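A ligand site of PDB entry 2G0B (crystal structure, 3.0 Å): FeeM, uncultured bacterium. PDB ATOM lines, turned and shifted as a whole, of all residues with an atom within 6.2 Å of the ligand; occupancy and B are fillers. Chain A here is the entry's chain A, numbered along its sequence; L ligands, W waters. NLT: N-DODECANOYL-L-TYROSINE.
The backbone NH (N) of Ile 143 lies within hydrogen-bond range of the backbone carbonyl oxygen (O) of Ile 173, at 3.1 Å. O of Tyr 29 sits at hydrogen-bond distance from N of Tyr 34, at 2.6 Å. O of Tyr 151 is in hydrogen-bond range of N of Phe 156, 3.0 Å away. The side-chain hydroxyl (OG) of Ser 142 sits at hydrogen-bond distance from the side-chain carboxylate (OE1) of Glu 96. The backbone NH (N) of Leu 139 sits at hydrogen-bond distance from the backbone carbonyl oxygen (O) of Leu 177, at 3.0 Å. The backbone carbonyl oxygen of Ala 170 lies within hydrogen-bond range of the backbone NH of Tyr 165 (2.9 Å). ND2 of Asn 144 sits at hydrogen-bond distance from OH of Tyr 34 (2.9 Å).
CE1 of Tyr 34 touches CE2 of the ligand (3.6 Å). Ile 64 touches the ligand. Val 97 touches the ligand (O to C3, 3.6 Å). Val 98 touches the ligand (CG2 to O, 3.1 Å). CD2 of Phe 124 touches C8 of the ligand, 3.7 Å away. Leu 128 touches the ligand. Ile 141 touches the ligand. Ile 143 touches the ligand (CG2 to C2, 3.5 Å). CE2 of Tyr 151 touches C6 of the ligand (3.5 Å). CE1 of Phe 156 touches C10 of the ligand, at 3.6 Å. Tyr 165 touches the ligand. Val 168 touches the ligand (CG1 to CE2, 3.5 Å). Ala 170 touches the ligand. Ala 172 touches the ligand (CB to CE1, 3.7 Å). Leu 177 touches the ligand. 21 residues have an atom within 4 Å of the ligand: Tyr 29, Tyr 34, Ile 64, Val 97, Val 98, Gln 99, Phe 100, Phe 124, Leu 128, Ile 141, Ser 142, Ile 143, Asn 144, Tyr 151, Phe 156, Tyr 165, Val 168, Ala 170, Pro 171, Ala 172 and Leu 177. The nearest printed residue that does not touch the ligand is Phe 40 (4.004 Å).
Water W1 lies within hydrogen-bond range of the backbone carbonyl oxygen (O) of Phe 100 (2.6 Å), an oxygen (OL) of the ligand (2.7 Å) and the side-chain hydroxyl (OH) of Tyr 29 (2.8 Å).
O2 of the ligand is in hydrogen-bond range of OH of Tyr 29, 2.4 Å away. An oxygen (OH) of the ligand is in hydrogen-bond range of the backbone carbonyl oxygen (O) of Pro 171 (2.8 Å). OL of the ligand is in hydrogen-bond range of N of Phe 100, 3.3 Å away. An oxygen (O) of the ligand lies within hydrogen-bond range of the backbone NH (N) of Gln 99, 3.1 Å away. The backbone carbonyl oxygen (O) of Ser 142 lies within hydrogen-bond range of a nitrogen (N) of the ligand (2.9 Å). The side-chain amide nitrogen (ND2) of Asn 144 lies within hydrogen-bond range of an oxygen (OH) of the ligand (2.7 Å).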
ATOM      1  N   VAL A  25       9.893 -28.626  18.062  1.00  0.00           N
ATOM      2  CA  VAL A  25       8.510 -28.156  18.203  1.00  0.00           C
ATOM      3  C   VAL A  25       8.306 -27.460  19.539  1.00  0.00           C
ATOM      4  O   VAL A  25       7.718 -26.387  19.598  1.00  0.00           O
ATOM      5  CB  VAL A  25       7.479 -29.293  18.016  1.00  0.00           C
ATOM      6  CG1 VAL A  25       6.067 -28.763  18.167  1.00  0.00           C
ATOM      7  CG2 VAL A  25       7.638 -29.936  16.659  1.00  0.00           C
ATOM      8  N   TYR A  29       7.601 -23.388  19.735  1.00  0.00           N
ATOM      9  CA  TYR A  29       6.291 -22.982  20.241  1.00  0.00           C
ATOM     10  C   TYR A  29       6.395 -22.140  21.513  1.00  0.00           C
ATOM     11  O   TYR A  29       5.609 -21.225  21.725  1.00  0.00           O
ATOM     12  CB  TYR A  29       5.388 -24.215  20.484  1.00  0.00           C
ATOM     13  CG  TYR A  29       4.818 -24.830  19.206  1.00  0.00           C
ATOM     14  CD1 TYR A  29       5.480 -24.691  17.983  1.00  0.00           C
ATOM     15  CD2 TYR A  29       3.615 -25.537  19.220  1.00  0.00           C
ATOM     16  CE1 TYR A  29       4.985 -25.243  16.819  1.00  0.00           C
ATOM     17  CE2 TYR A  29       3.091 -26.099  18.044  1.00  0.00           C
ATOM     18  CZ  TYR A  29       3.787 -25.937  16.844  1.00  0.00           C
ATOM     19  OH  TYR A  29       3.331 -26.472  15.648  1.00  0.00           O
ATOM     20  N   TYR A  34       3.269 -20.190  22.124  1.00  0.00           N
ATOM     21  CA  TYR A  34       2.243 -21.230  21.988  1.00  0.00           C
ATOM     22  C   TYR A  34       2.385 -22.218  23.128  1.00  0.00           C
ATOM     23  O   TYR A  34       3.492 -22.485  23.588  1.00  0.00           O
ATOM     24  CB  TYR A  34       2.422 -21.977  20.680  1.00  0.00           C
ATOM     25  CG  TYR A  34       2.362 -21.142  19.413  1.00  0.00           C
ATOM     26  CD1 TYR A  34       2.936 -21.607  18.234  1.00  0.00           C
ATOM     27  CD2 TYR A  34       1.723 -19.889  19.377  1.00  0.00           C
ATOM     28  CE1 TYR A  34       2.902 -20.874  17.067  1.00  0.00           C
ATOM     29  CE2 TYR A  34       1.681 -19.146  18.203  1.00  0.00           C
ATOM     30  CZ  TYR A  34       2.276 -19.649  17.048  1.00  0.00           C
ATOM     31  OH  TYR A  34       2.274 -18.941  15.885  1.00  0.00           O
ATOM     32  N   PHE A  40      -0.683 -33.788  21.099  1.00  0.00           N
ATOM     33  CA  PHE A  40       0.014 -33.818  19.815  1.00  0.00           C
ATOM     34  C   PHE A  40       1.028 -34.941  19.770  1.00  0.00           C
ATOM     35  O   PHE A  40       1.157 -35.617  18.758  1.00  0.00           O
ATOM     36  CB  PHE A  40       0.702 -32.486  19.547  1.00  0.00           C
ATOM     37  CG  PHE A  40      -0.178 -31.456  18.895  1.00  0.00           C
ATOM     38  CD1 PHE A  40      -0.458 -30.254  19.534  1.00  0.00           C
ATOM     39  CD2 PHE A  40      -0.711 -31.685  17.627  1.00  0.00           C
ATOM     40  CE1 PHE A  40      -1.256 -29.300  18.920  1.00  0.00           C
ATOM     41  CE2 PHE A  40      -1.513 -30.727  17.021  1.00  0.00           C
ATOM     42  CZ  PHE A  40      -1.785 -29.535  17.667  1.00  0.00           C
ATOM     43  N   ILE A  64       8.090 -31.869  10.234  1.00  0.00           N
ATOM     44  CA  ILE A  64       6.663 -31.770   9.899  1.00  0.00           C
ATOM     45  C   ILE A  64       6.038 -33.152   9.991  1.00  0.00           C
ATOM     46  O   ILE A  64       6.663 -34.147   9.636  1.00  0.00           O
ATOM     47  CB  ILE A  64       6.449 -31.113   8.480  1.00  0.00           C
ATOM     48  CG1 ILE A  64       5.022 -30.594   8.327  1.00  0.00           C
ATOM     49  CG2 ILE A  64       6.795 -32.077   7.346  1.00  0.00           C
ATOM     50  CD1 ILE A  64       4.856 -29.514   7.271  1.00  0.00           C
ATOM     51  N   GLU A  96      -4.490 -34.335   8.365  1.00  0.00           N
ATOM     52  CA  GLU A  96      -4.089 -33.034   8.864  1.00  0.00           C
ATOM     53  C   GLU A  96      -2.578 -32.957   8.940  1.00  0.00           C
ATOM     54  O   GLU A  96      -1.945 -33.849   9.500  1.00  0.00           O
ATOM     55  CB  GLU A  96      -4.734 -32.750  10.216  1.00  0.00           C
ATOM     56  CG  GLU A  96      -4.056 -31.625  10.981  1.00  0.00           C
ATOM     57  CD  GLU A  96      -4.937 -30.950  12.033  1.00  0.00           C
ATOM     58  OE1 GLU A  96      -4.715 -29.741  12.299  1.00  0.00           O
ATOM     59  OE2 GLU A  96      -5.823 -31.629  12.610  1.00  0.00           O
ATOM     60  N   VAL A  97      -2.009 -31.924   8.333  1.00  0.00           N
ATOM     61  CA  VAL A  97      -0.585 -31.668   8.439  1.00  0.00           C
ATOM     62  C   VAL A  97      -0.336 -30.863   9.698  1.00  0.00           C
ATOM     63  O   VAL A  97      -0.922 -29.782   9.898  1.00  0.00           O
ATOM     64  CB  VAL A  97      -0.040 -30.922   7.216  1.00  0.00           C
ATOM     65  CG1 VAL A  97       1.450 -30.934   7.229  1.00  0.00           C
ATOM     66  CG2 VAL A  97      -0.545 -31.556   5.945  1.00  0.00           C
ATOM     67  N   VAL A  98       0.562 -31.368  10.538  1.00  0.00           N
ATOM     68  CA  VAL A  98       0.635 -30.945  11.912  1.00  0.00           C
ATOM     69  C   VAL A  98       2.108 -30.884  12.430  1.00  0.00           C
ATOM     70  O   VAL A  98       3.012 -31.470  11.813  1.00  0.00           O
ATOM     71  CB  VAL A  98      -0.257 -31.894  12.753  1.00  0.00           C
ATOM     72  CG1 VAL A  98       0.548 -32.780  13.683  1.00  0.00           C
ATOM     73  CG2 VAL A  98      -1.316 -31.142  13.463  1.00  0.00           C
ATOM     74  N   GLN A  99       2.338 -30.125  13.515  1.00  0.00           N
ATOM     75  CA  GLN A  99       3.653 -30.025  14.195  1.00  0.00           C
ATOM     76  C   GLN A  99       4.810 -29.602  13.274  1.00  0.00           C
ATOM     77  O   GLN A  99       5.917 -30.155  13.323  1.00  0.00           O
ATOM     78  CB  GLN A  99       4.011 -31.320  14.967  1.00  0.00           C
ATOM     79  CG  GLN A  99       3.023 -31.721  16.058  1.00  0.00           C
ATOM     80  CD  GLN A  99       3.313 -31.074  17.409  1.00  0.00           C
ATOM     81  OE1 GLN A  99       2.736 -30.031  17.738  1.00  0.00           O
ATOM     82  NE2 GLN A  99       4.149 -31.716  18.218  1.00  0.00           N
ATOM     83  N   PHE A 100       4.527 -28.629  12.409  1.00  0.00           N
ATOM     84  CA  PHE A 100       5.535 -28.039  11.549  1.00  0.00           C
ATOM     85  C   PHE A 100       6.343 -27.034  12.370  1.00  0.00           C
ATOM     86  O   PHE A 100       5.781 -26.106  12.965  1.00  0.00           O
ATOM     87  CB  PHE A 100       4.867 -27.365  10.352  1.00  0.00           C
ATOM     88  CG  PHE A 100       5.788 -26.533   9.522  1.00  0.00           C
ATOM     89  CD1 PHE A 100       7.003 -27.041   9.086  1.00  0.00           C
ATOM     90  CD2 PHE A 100       5.449 -25.253   9.150  1.00  0.00           C
ATOM     91  CE1 PHE A 100       7.847 -26.280   8.335  1.00  0.00           C
ATOM     92  CE2 PHE A 100       6.290 -24.485   8.383  1.00  0.00           C
ATOM     93  CZ  PHE A 100       7.489 -24.994   7.975  1.00  0.00           C
ATOM     94  N   ALA A 101       7.651 -27.243  12.404  1.00  0.00           N
ATOM     95  CA  ALA A 101       8.551 -26.394  13.165  1.00  0.00           C
ATOM     96  C   ALA A 101       9.935 -26.413  12.582  1.00  0.00           C
ATOM     97  O   ALA A 101      10.379 -27.444  12.079  1.00  0.00           O
ATOM     98  CB  ALA A 101       8.587 -26.842  14.636  1.00  0.00           C
ATOM     99  N   PHE A 124       7.748 -30.008   2.472  1.00  0.00           N
ATOM    100  CA  PHE A 124       6.423 -29.922   1.850  1.00  0.00           C
ATOM    101  C   PHE A 124       6.261 -30.907   0.707  1.00  0.00           C
ATOM    102  O   PHE A 124       5.215 -31.527   0.560  1.00  0.00           O
ATOM    103  CB  PHE A 124       6.132 -28.509   1.347  1.00  0.00           C
ATOM    104  CG  PHE A 124       5.954 -27.485   2.445  1.00  0.00           C
ATOM    105  CD1 PHE A 124       6.073 -26.126   2.152  1.00  0.00           C
ATOM    106  CD2 PHE A 124       5.661 -27.868   3.745  1.00  0.00           C
ATOM    107  CE1 PHE A 124       5.905 -25.175   3.150  1.00  0.00           C
ATOM    108  CE2 PHE A 124       5.490 -26.905   4.748  1.00  0.00           C
ATOM    109  CZ  PHE A 124       5.615 -25.570   4.445  1.00  0.00           C
ATOM    110  N   THR A 125       7.309 -31.048  -0.114  1.00  0.00           N
ATOM    111  CA  THR A 125       7.295 -32.023  -1.216  1.00  0.00           C
ATOM    112  C   THR A 125       7.056 -33.432  -0.684  1.00  0.00           C
ATOM    113  O   THR A 125       6.327 -34.223  -1.300  1.00  0.00           O
ATOM    114  CB  THR A 125       8.611 -32.006  -2.007  1.00  0.00           C
ATOM    115  OG1 THR A 125       9.064 -30.669  -2.201  1.00  0.00           O
ATOM    116  CG2 THR A 125       8.335 -32.463  -3.385  1.00  0.00           C
ATOM    117  N   VAL A 127       5.434 -34.164   2.076  1.00  0.00           N
ATOM    118  CA  VAL A 127       4.018 -34.221   2.489  1.00  0.00           C
ATOM    119  C   VAL A 127       3.109 -34.412   1.263  1.00  0.00           C
ATOM    120  O   VAL A 127       2.216 -35.261   1.274  1.00  0.00           O
ATOM    121  CB  VAL A 127       3.571 -32.948   3.285  1.00  0.00           C
ATOM    122  CG1 VAL A 127       2.063 -32.954   3.533  1.00  0.00           C
ATOM    123  CG2 VAL A 127       4.314 -32.847   4.586  1.00  0.00           C
ATOM    124  N   LEU A 128       3.364 -33.626   0.213  1.00  0.00           N
ATOM    125  CA  LEU A 128       2.608 -33.718  -1.025  1.00  0.00           C
ATOM    126  C   LEU A 128       2.719 -35.111  -1.687  1.00  0.00           C
ATOM    127  O   LEU A 128       1.701 -35.691  -2.049  1.00  0.00           O
ATOM    128  CB  LEU A 128       3.018 -32.621  -2.008  1.00  0.00           C
ATOM    129  CG  LEU A 128       2.287 -32.579  -3.354  1.00  0.00           C
ATOM    130  CD1 LEU A 128       0.844 -32.144  -3.185  1.00  0.00           C
ATOM    131  CD2 LEU A 128       2.994 -31.694  -4.334  1.00  0.00           C
ATOM    132  N   LEU A 139      -6.167 -32.296   2.212  1.00  0.00           N
ATOM    133  CA  LEU A 139      -5.081 -32.038   3.139  1.00  0.00           C
ATOM    134  C   LEU A 139      -5.438 -30.809   3.978  1.00  0.00           C
ATOM    135  O   LEU A 139      -5.485 -29.706   3.472  1.00  0.00           O
ATOM    136  CB  LEU A 139      -3.802 -31.784   2.349  1.00  0.00           C
ATOM    137  CG  LEU A 139      -2.482 -32.331   2.862  1.00  0.00           C
ATOM    138  CD1 LEU A 139      -2.634 -33.709   3.443  1.00  0.00           C
ATOM    139  CD2 LEU A 139      -1.510 -32.373   1.723  1.00  0.00           C
ATOM    140  N   ILE A 141      -5.135 -28.003   7.267  1.00  0.00           N
ATOM    141  CA  ILE A 141      -4.174 -27.294   8.126  1.00  0.00           C
ATOM    142  C   ILE A 141      -4.841 -26.293   9.033  1.00  0.00           C
ATOM    143  O   ILE A 141      -5.770 -25.588   8.618  1.00  0.00           O
ATOM    144  CB  ILE A 141      -3.032 -26.570   7.291  1.00  0.00           C
ATOM    145  CG1 ILE A 141      -3.618 -25.719   6.170  1.00  0.00           C
ATOM    146  CG2 ILE A 141      -2.004 -27.570   6.764  1.00  0.00           C
ATOM    147  CD1 ILE A 141      -2.638 -24.748   5.563  1.00  0.00           C
ATOM    148  N   SER A 142      -4.395 -26.217  10.273  1.00  0.00           N
ATOM    149  CA  SER A 142      -4.819 -25.135  11.153  1.00  0.00           C
ATOM    150  C   SER A 142      -3.592 -24.331  11.488  1.00  0.00           C
ATOM    151  O   SER A 142      -2.648 -24.841  12.079  1.00  0.00           O
ATOM    152  CB  SER A 142      -5.513 -25.673  12.396  1.00  0.00           C
ATOM    153  OG  SER A 142      -4.676 -26.570  13.084  1.00  0.00           O
ATOM    154  N   ILE A 143      -3.603 -23.086  11.058  1.00  0.00           N
ATOM    155  CA  ILE A 143      -2.405 -22.256  11.031  1.00  0.00           C
ATOM    156  C   ILE A 143      -2.594 -20.933  11.772  1.00  0.00           C
ATOM    157  O   ILE A 143      -3.702 -20.397  11.848  1.00  0.00           O
ATOM    158  CB  ILE A 143      -2.011 -21.966   9.568  1.00  0.00           C
ATOM    159  CG1 ILE A 143      -3.264 -21.679   8.732  1.00  0.00           C
ATOM    160  CG2 ILE A 143      -1.275 -23.120   8.973  1.00  0.00           C
ATOM    161  CD1 ILE A 143      -3.158 -20.443   7.925  1.00  0.00           C
ATOM    162  N   ASN A 144      -1.491 -20.395  12.292  1.00  0.00           N
ATOM    163  CA  ASN A 144      -1.505 -19.070  12.840  1.00  0.00           C
ATOM    164  C   ASN A 144      -1.818 -18.064  11.742  1.00  0.00           C
ATOM    165  O   ASN A 144      -1.239 -18.148  10.652  1.00  0.00           O
ATOM    166  CB  ASN A 144      -0.157 -18.751  13.458  1.00  0.00           C
ATOM    167  CG  ASN A 144      -0.196 -17.541  14.323  1.00  0.00           C
ATOM    168  OD1 ASN A 144      -0.125 -16.422  13.829  1.00  0.00           O
ATOM    169  ND2 ASN A 144      -0.344 -17.746  15.626  1.00  0.00           N
ATOM    170  N   PRO A 145      -2.720 -17.113  12.020  1.00  0.00           N
ATOM    171  CA  PRO A 145      -3.145 -16.115  11.020  1.00  0.00           C
ATOM    172  C   PRO A 145      -2.017 -15.379  10.292  1.00  0.00           C
ATOM    173  O   PRO A 145      -2.301 -14.756   9.268  1.00  0.00           O
ATOM    174  CB  PRO A 145      -3.953 -15.124  11.852  1.00  0.00           C
ATOM    175  CG  PRO A 145      -4.447 -15.904  12.983  1.00  0.00           C
ATOM    176  CD  PRO A 145      -3.438 -16.933  13.298  1.00  0.00           C
ATOM    177  N   TYR A 151      -0.147 -19.697   2.711  1.00  0.00           N
ATOM    178  CA  TYR A 151      -0.780 -20.966   2.383  1.00  0.00           C
ATOM    179  C   TYR A 151      -1.911 -20.822   1.367  1.00  0.00           C
ATOM    180  O   TYR A 151      -2.235 -21.773   0.662  1.00  0.00           O
ATOM    181  CB  TYR A 151      -1.241 -21.667   3.660  1.00  0.00           C
ATOM    182  CG  TYR A 151      -0.093 -22.126   4.503  1.00  0.00           C
ATOM    183  CD1 TYR A 151       0.114 -21.593   5.778  1.00  0.00           C
ATOM    184  CD2 TYR A 151       0.819 -23.063   4.021  1.00  0.00           C
ATOM    185  CE1 TYR A 151       1.189 -21.989   6.545  1.00  0.00           C
ATOM    186  CE2 TYR A 151       1.899 -23.462   4.779  1.00  0.00           C
ATOM    187  CZ  TYR A 151       2.075 -22.927   6.048  1.00  0.00           C
ATOM    188  OH  TYR A 151       3.140 -23.326   6.834  1.00  0.00           O
ATOM    189  N   LEU A 154      -0.179 -21.140  -1.809  1.00  0.00           N
ATOM    190  CA  LEU A 154       0.061 -22.576  -1.999  1.00  0.00           C
ATOM    191  C   LEU A 154      -1.199 -23.350  -2.399  1.00  0.00           C
ATOM    192  O   LEU A 154      -1.123 -24.563  -2.666  1.00  0.00           O
ATOM    193  CB  LEU A 154       0.651 -23.200  -0.744  1.00  0.00           C
ATOM    194  CG  LEU A 154       2.119 -22.983  -0.383  1.00  0.00           C
ATOM    195  CD1 LEU A 154       2.624 -24.172   0.432  1.00  0.00           C
ATOM    196  CD2 LEU A 154       2.985 -22.769  -1.604  1.00  0.00           C
ATOM    197  N   PHE A 156      -4.295 -23.547  -0.678  1.00  0.00           N
ATOM    198  CA  PHE A 156      -5.210 -23.918   0.406  1.00  0.00           C
ATOM    199  C   PHE A 156      -6.369 -22.937   0.506  1.00  0.00           C
ATOM    200  O   PHE A 156      -6.173 -21.721   0.634  1.00  0.00           O
ATOM    201  CB  PHE A 156      -4.473 -23.960   1.719  1.00  0.00           C
ATOM    202  CG  PHE A 156      -3.600 -25.158   1.888  1.00  0.00           C
ATOM    203  CD1 PHE A 156      -2.286 -25.134   1.454  1.00  0.00           C
ATOM    204  CD2 PHE A 156      -4.066 -26.288   2.540  1.00  0.00           C
ATOM    205  CE1 PHE A 156      -1.458 -26.224   1.643  1.00  0.00           C
ATOM    206  CE2 PHE A 156      -3.252 -27.376   2.732  1.00  0.00           C
ATOM    207  CZ  PHE A 156      -1.941 -27.346   2.282  1.00  0.00           C
ATOM    208  N   TYR A 165      -7.717 -21.547  19.239  1.00  0.00           N
ATOM    209  CA  TYR A 165      -7.318 -22.945  19.339  1.00  0.00           C
ATOM    210  C   TYR A 165      -6.817 -23.185  20.751  1.00  0.00           C
ATOM    211  O   TYR A 165      -5.693 -22.806  21.091  1.00  0.00           O
ATOM    212  CB  TYR A 165      -6.232 -23.236  18.307  1.00  0.00           C
ATOM    213  CG  TYR A 165      -6.003 -24.712  17.970  1.00  0.00           C
ATOM    214  CD1 TYR A 165      -6.799 -25.718  18.513  1.00  0.00           C
ATOM    215  CD2 TYR A 165      -4.962 -25.096  17.103  1.00  0.00           C
ATOM    216  CE1 TYR A 165      -6.589 -27.062  18.189  1.00  0.00           C
ATOM    217  CE2 TYR A 165      -4.742 -26.430  16.780  1.00  0.00           C
ATOM    218  CZ  TYR A 165      -5.552 -27.402  17.327  1.00  0.00           C
ATOM    219  OH  TYR A 165      -5.324 -28.713  17.013  1.00  0.00           O
ATOM    220  N   VAL A 168      -3.406 -24.948  21.648  1.00  0.00           N
ATOM    221  CA  VAL A 168      -2.205 -24.161  21.470  1.00  0.00           C
ATOM    222  C   VAL A 168      -2.242 -22.816  22.226  1.00  0.00           C
ATOM    223  O   VAL A 168      -1.200 -22.171  22.421  1.00  0.00           O
ATOM    224  CB  VAL A 168      -1.936 -23.917  19.967  1.00  0.00           C
ATOM    225  CG1 VAL A 168      -0.620 -23.331  19.771  1.00  0.00           C
ATOM    226  CG2 VAL A 168      -2.007 -25.222  19.220  1.00  0.00           C
ATOM    227  N   ALA A 170      -3.681 -20.046  21.078  1.00  0.00           N
ATOM    228  CA  ALA A 170      -3.332 -19.091  20.042  1.00  0.00           C
ATOM    229  C   ALA A 170      -4.458 -19.093  18.998  1.00  0.00           C
ATOM    230  O   ALA A 170      -5.229 -20.061  18.916  1.00  0.00           O
ATOM    231  CB  ALA A 170      -2.011 -19.471  19.412  1.00  0.00           C
ATOM    232  N   PRO A 171      -4.599 -17.999  18.227  1.00  0.00           N
ATOM    233  CA  PRO A 171      -5.620 -17.939  17.158  1.00  0.00           C
ATOM    234  C   PRO A 171      -5.300 -18.898  16.032  1.00  0.00           C
ATOM    235  O   PRO A 171      -4.118 -19.211  15.818  1.00  0.00           O
ATOM    236  CB  PRO A 171      -5.501 -16.503  16.658  1.00  0.00           C
ATOM    237  CG  PRO A 171      -4.785 -15.775  17.711  1.00  0.00           C
ATOM    238  CD  PRO A 171      -3.849 -16.734  18.344  1.00  0.00           C
ATOM    239  N   ALA A 172      -6.325 -19.349  15.306  1.00  0.00           N
ATOM    240  CA  ALA A 172      -6.134 -20.261  14.163  1.00  0.00           C
ATOM    241  C   ALA A 172      -7.250 -20.127  13.122  1.00  0.00           C
ATOM    242  O   ALA A 172      -8.408 -19.902  13.478  1.00  0.00           O
ATOM    243  CB  ALA A 172      -6.031 -21.708  14.634  1.00  0.00           C
ATOM    244  N   ILE A 173      -6.882 -20.256  11.835  1.00  0.00           N
ATOM    245  CA  ILE A 173      -7.873 -20.502  10.777  1.00  0.00           C
ATOM    246  C   ILE A 173      -7.620 -21.860  10.169  1.00  0.00           C
ATOM    247  O   ILE A 173      -6.487 -22.346  10.171  1.00  0.00           O
ATOM    248  CB  ILE A 173      -7.873 -19.396   9.647  1.00  0.00           C
ATOM    249  CG1 ILE A 173      -6.495 -19.190   9.073  1.00  0.00           C
ATOM    250  CG2 ILE A 173      -8.309 -18.065  10.175  1.00  0.00           C
ATOM    251  CD1 ILE A 173      -5.980 -17.802   9.387  1.00  0.00           C
ATOM    252  N   LEU A 177      -6.790 -28.323   1.145  1.00  0.00           N
ATOM    253  CA  LEU A 177      -6.452 -28.401  -0.274  1.00  0.00           C
ATOM    254  C   LEU A 177      -6.899 -29.746  -0.877  1.00  0.00           C
ATOM    255  O   LEU A 177      -6.629 -30.815  -0.320  1.00  0.00           O
ATOM    256  CB  LEU A 177      -4.946 -28.184  -0.480  1.00  0.00           C
ATOM    257  CG  LEU A 177      -4.309 -28.676  -1.795  1.00  0.00           C
ATOM    258  CD1 LEU A 177      -4.627 -27.727  -2.947  1.00  0.00           C
ATOM    259  CD2 LEU A 177      -2.822 -28.844  -1.630  1.00  0.00           C
ATOM    260  N   TRP A 182      -4.420 -30.488  -7.243  1.00  0.00           N
ATOM    261  CA  TRP A 182      -3.734 -29.426  -6.510  1.00  0.00           C
ATOM    262  C   TRP A 182      -3.226 -28.297  -7.403  1.00  0.00           C
ATOM    263  O   TRP A 182      -3.165 -27.142  -6.967  1.00  0.00           O
ATOM    264  CB  TRP A 182      -2.585 -30.012  -5.669  1.00  0.00           C
ATOM    265  CG  TRP A 182      -1.464 -30.683  -6.470  1.00  0.00           C
ATOM    266  CD1 TRP A 182      -1.337 -32.006  -6.728  1.00  0.00           C
ATOM    267  CD2 TRP A 182      -0.322 -30.046  -7.057  1.00  0.00           C
ATOM    268  NE1 TRP A 182      -0.189 -32.241  -7.459  1.00  0.00           N
ATOM    269  CE2 TRP A 182       0.457 -31.054  -7.671  1.00  0.00           C
ATOM    270  CE3 TRP A 182       0.141 -28.717  -7.124  1.00  0.00           C
ATOM    271  CZ2 TRP A 182       1.648 -30.780  -8.362  1.00  0.00           C
ATOM    272  CZ3 TRP A 182       1.330 -28.452  -7.812  1.00  0.00           C
ATOM    273  CH2 TRP A 182       2.061 -29.482  -8.420  1.00  0.00           C
HETATM  274  N   NLT L   1      -0.072 -25.803  12.949  1.00  0.00           N
HETATM  275  C1  NLT L   1       0.903 -26.016  12.055  1.00  0.00           C
HETATM  276  OL  NLT L   1       2.010 -26.457  12.350  1.00  0.00           O
HETATM  277  C2  NLT L   1       0.568 -25.664  10.609  1.00  0.00           C
HETATM  278  C3  NLT L   1       1.041 -26.732   9.620  1.00  0.00           C
HETATM  279  C4  NLT L   1       1.213 -26.154   8.204  1.00  0.00           C
HETATM  280  C5  NLT L   1       1.709 -27.216   7.213  1.00  0.00           C
HETATM  281  C6  NLT L   1       1.552 -26.788   5.755  1.00  0.00           C
HETATM  282  C7  NLT L   1       1.710 -27.968   4.800  1.00  0.00           C
HETATM  283  C8  NLT L   1       2.029 -27.505   3.388  1.00  0.00           C
HETATM  284  C9  NLT L   1       2.126 -28.659   2.378  1.00  0.00           C
HETATM  285  C10 NLT L   1       1.478 -28.221   1.064  1.00  0.00           C
HETATM  286  C11 NLT L   1       1.395 -29.320   0.006  1.00  0.00           C
HETATM  287  C12 NLT L   1       0.993 -28.709  -1.343  1.00  0.00           C
HETATM  288  CA  NLT L   1       0.067 -25.967  14.397  1.00  0.00           C
HETATM  289  CB  NLT L   1      -1.233 -25.604  15.092  1.00  0.00           C
HETATM  290  CG  NLT L   1      -1.293 -24.117  15.411  1.00  0.00           C
HETATM  291  CD2 NLT L   1      -0.329 -23.537  16.223  1.00  0.00           C
HETATM  292  CE2 NLT L   1      -0.382 -22.185  16.512  1.00  0.00           C
HETATM  293  CZ  NLT L   1      -1.406 -21.420  15.998  1.00  0.00           C
HETATM  294  CE1 NLT L   1      -2.378 -22.000  15.181  1.00  0.00           C
HETATM  295  CD1 NLT L   1      -2.315 -23.342  14.894  1.00  0.00           C
HETATM  296  OH  NLT L   1      -1.466 -20.122  16.279  1.00  0.00           O
HETATM  297  C   NLT L   1       0.386 -27.387  14.785  1.00  0.00           C
HETATM  298  O   NLT L   1      -0.150 -28.311  14.133  1.00  0.00           O
HETATM  299  O2  NLT L   1       1.167 -27.596  15.753  1.00  0.00           O
HETATM  300  O   HOH W   1       3.668 -24.727  13.508  1.00  0.00           O
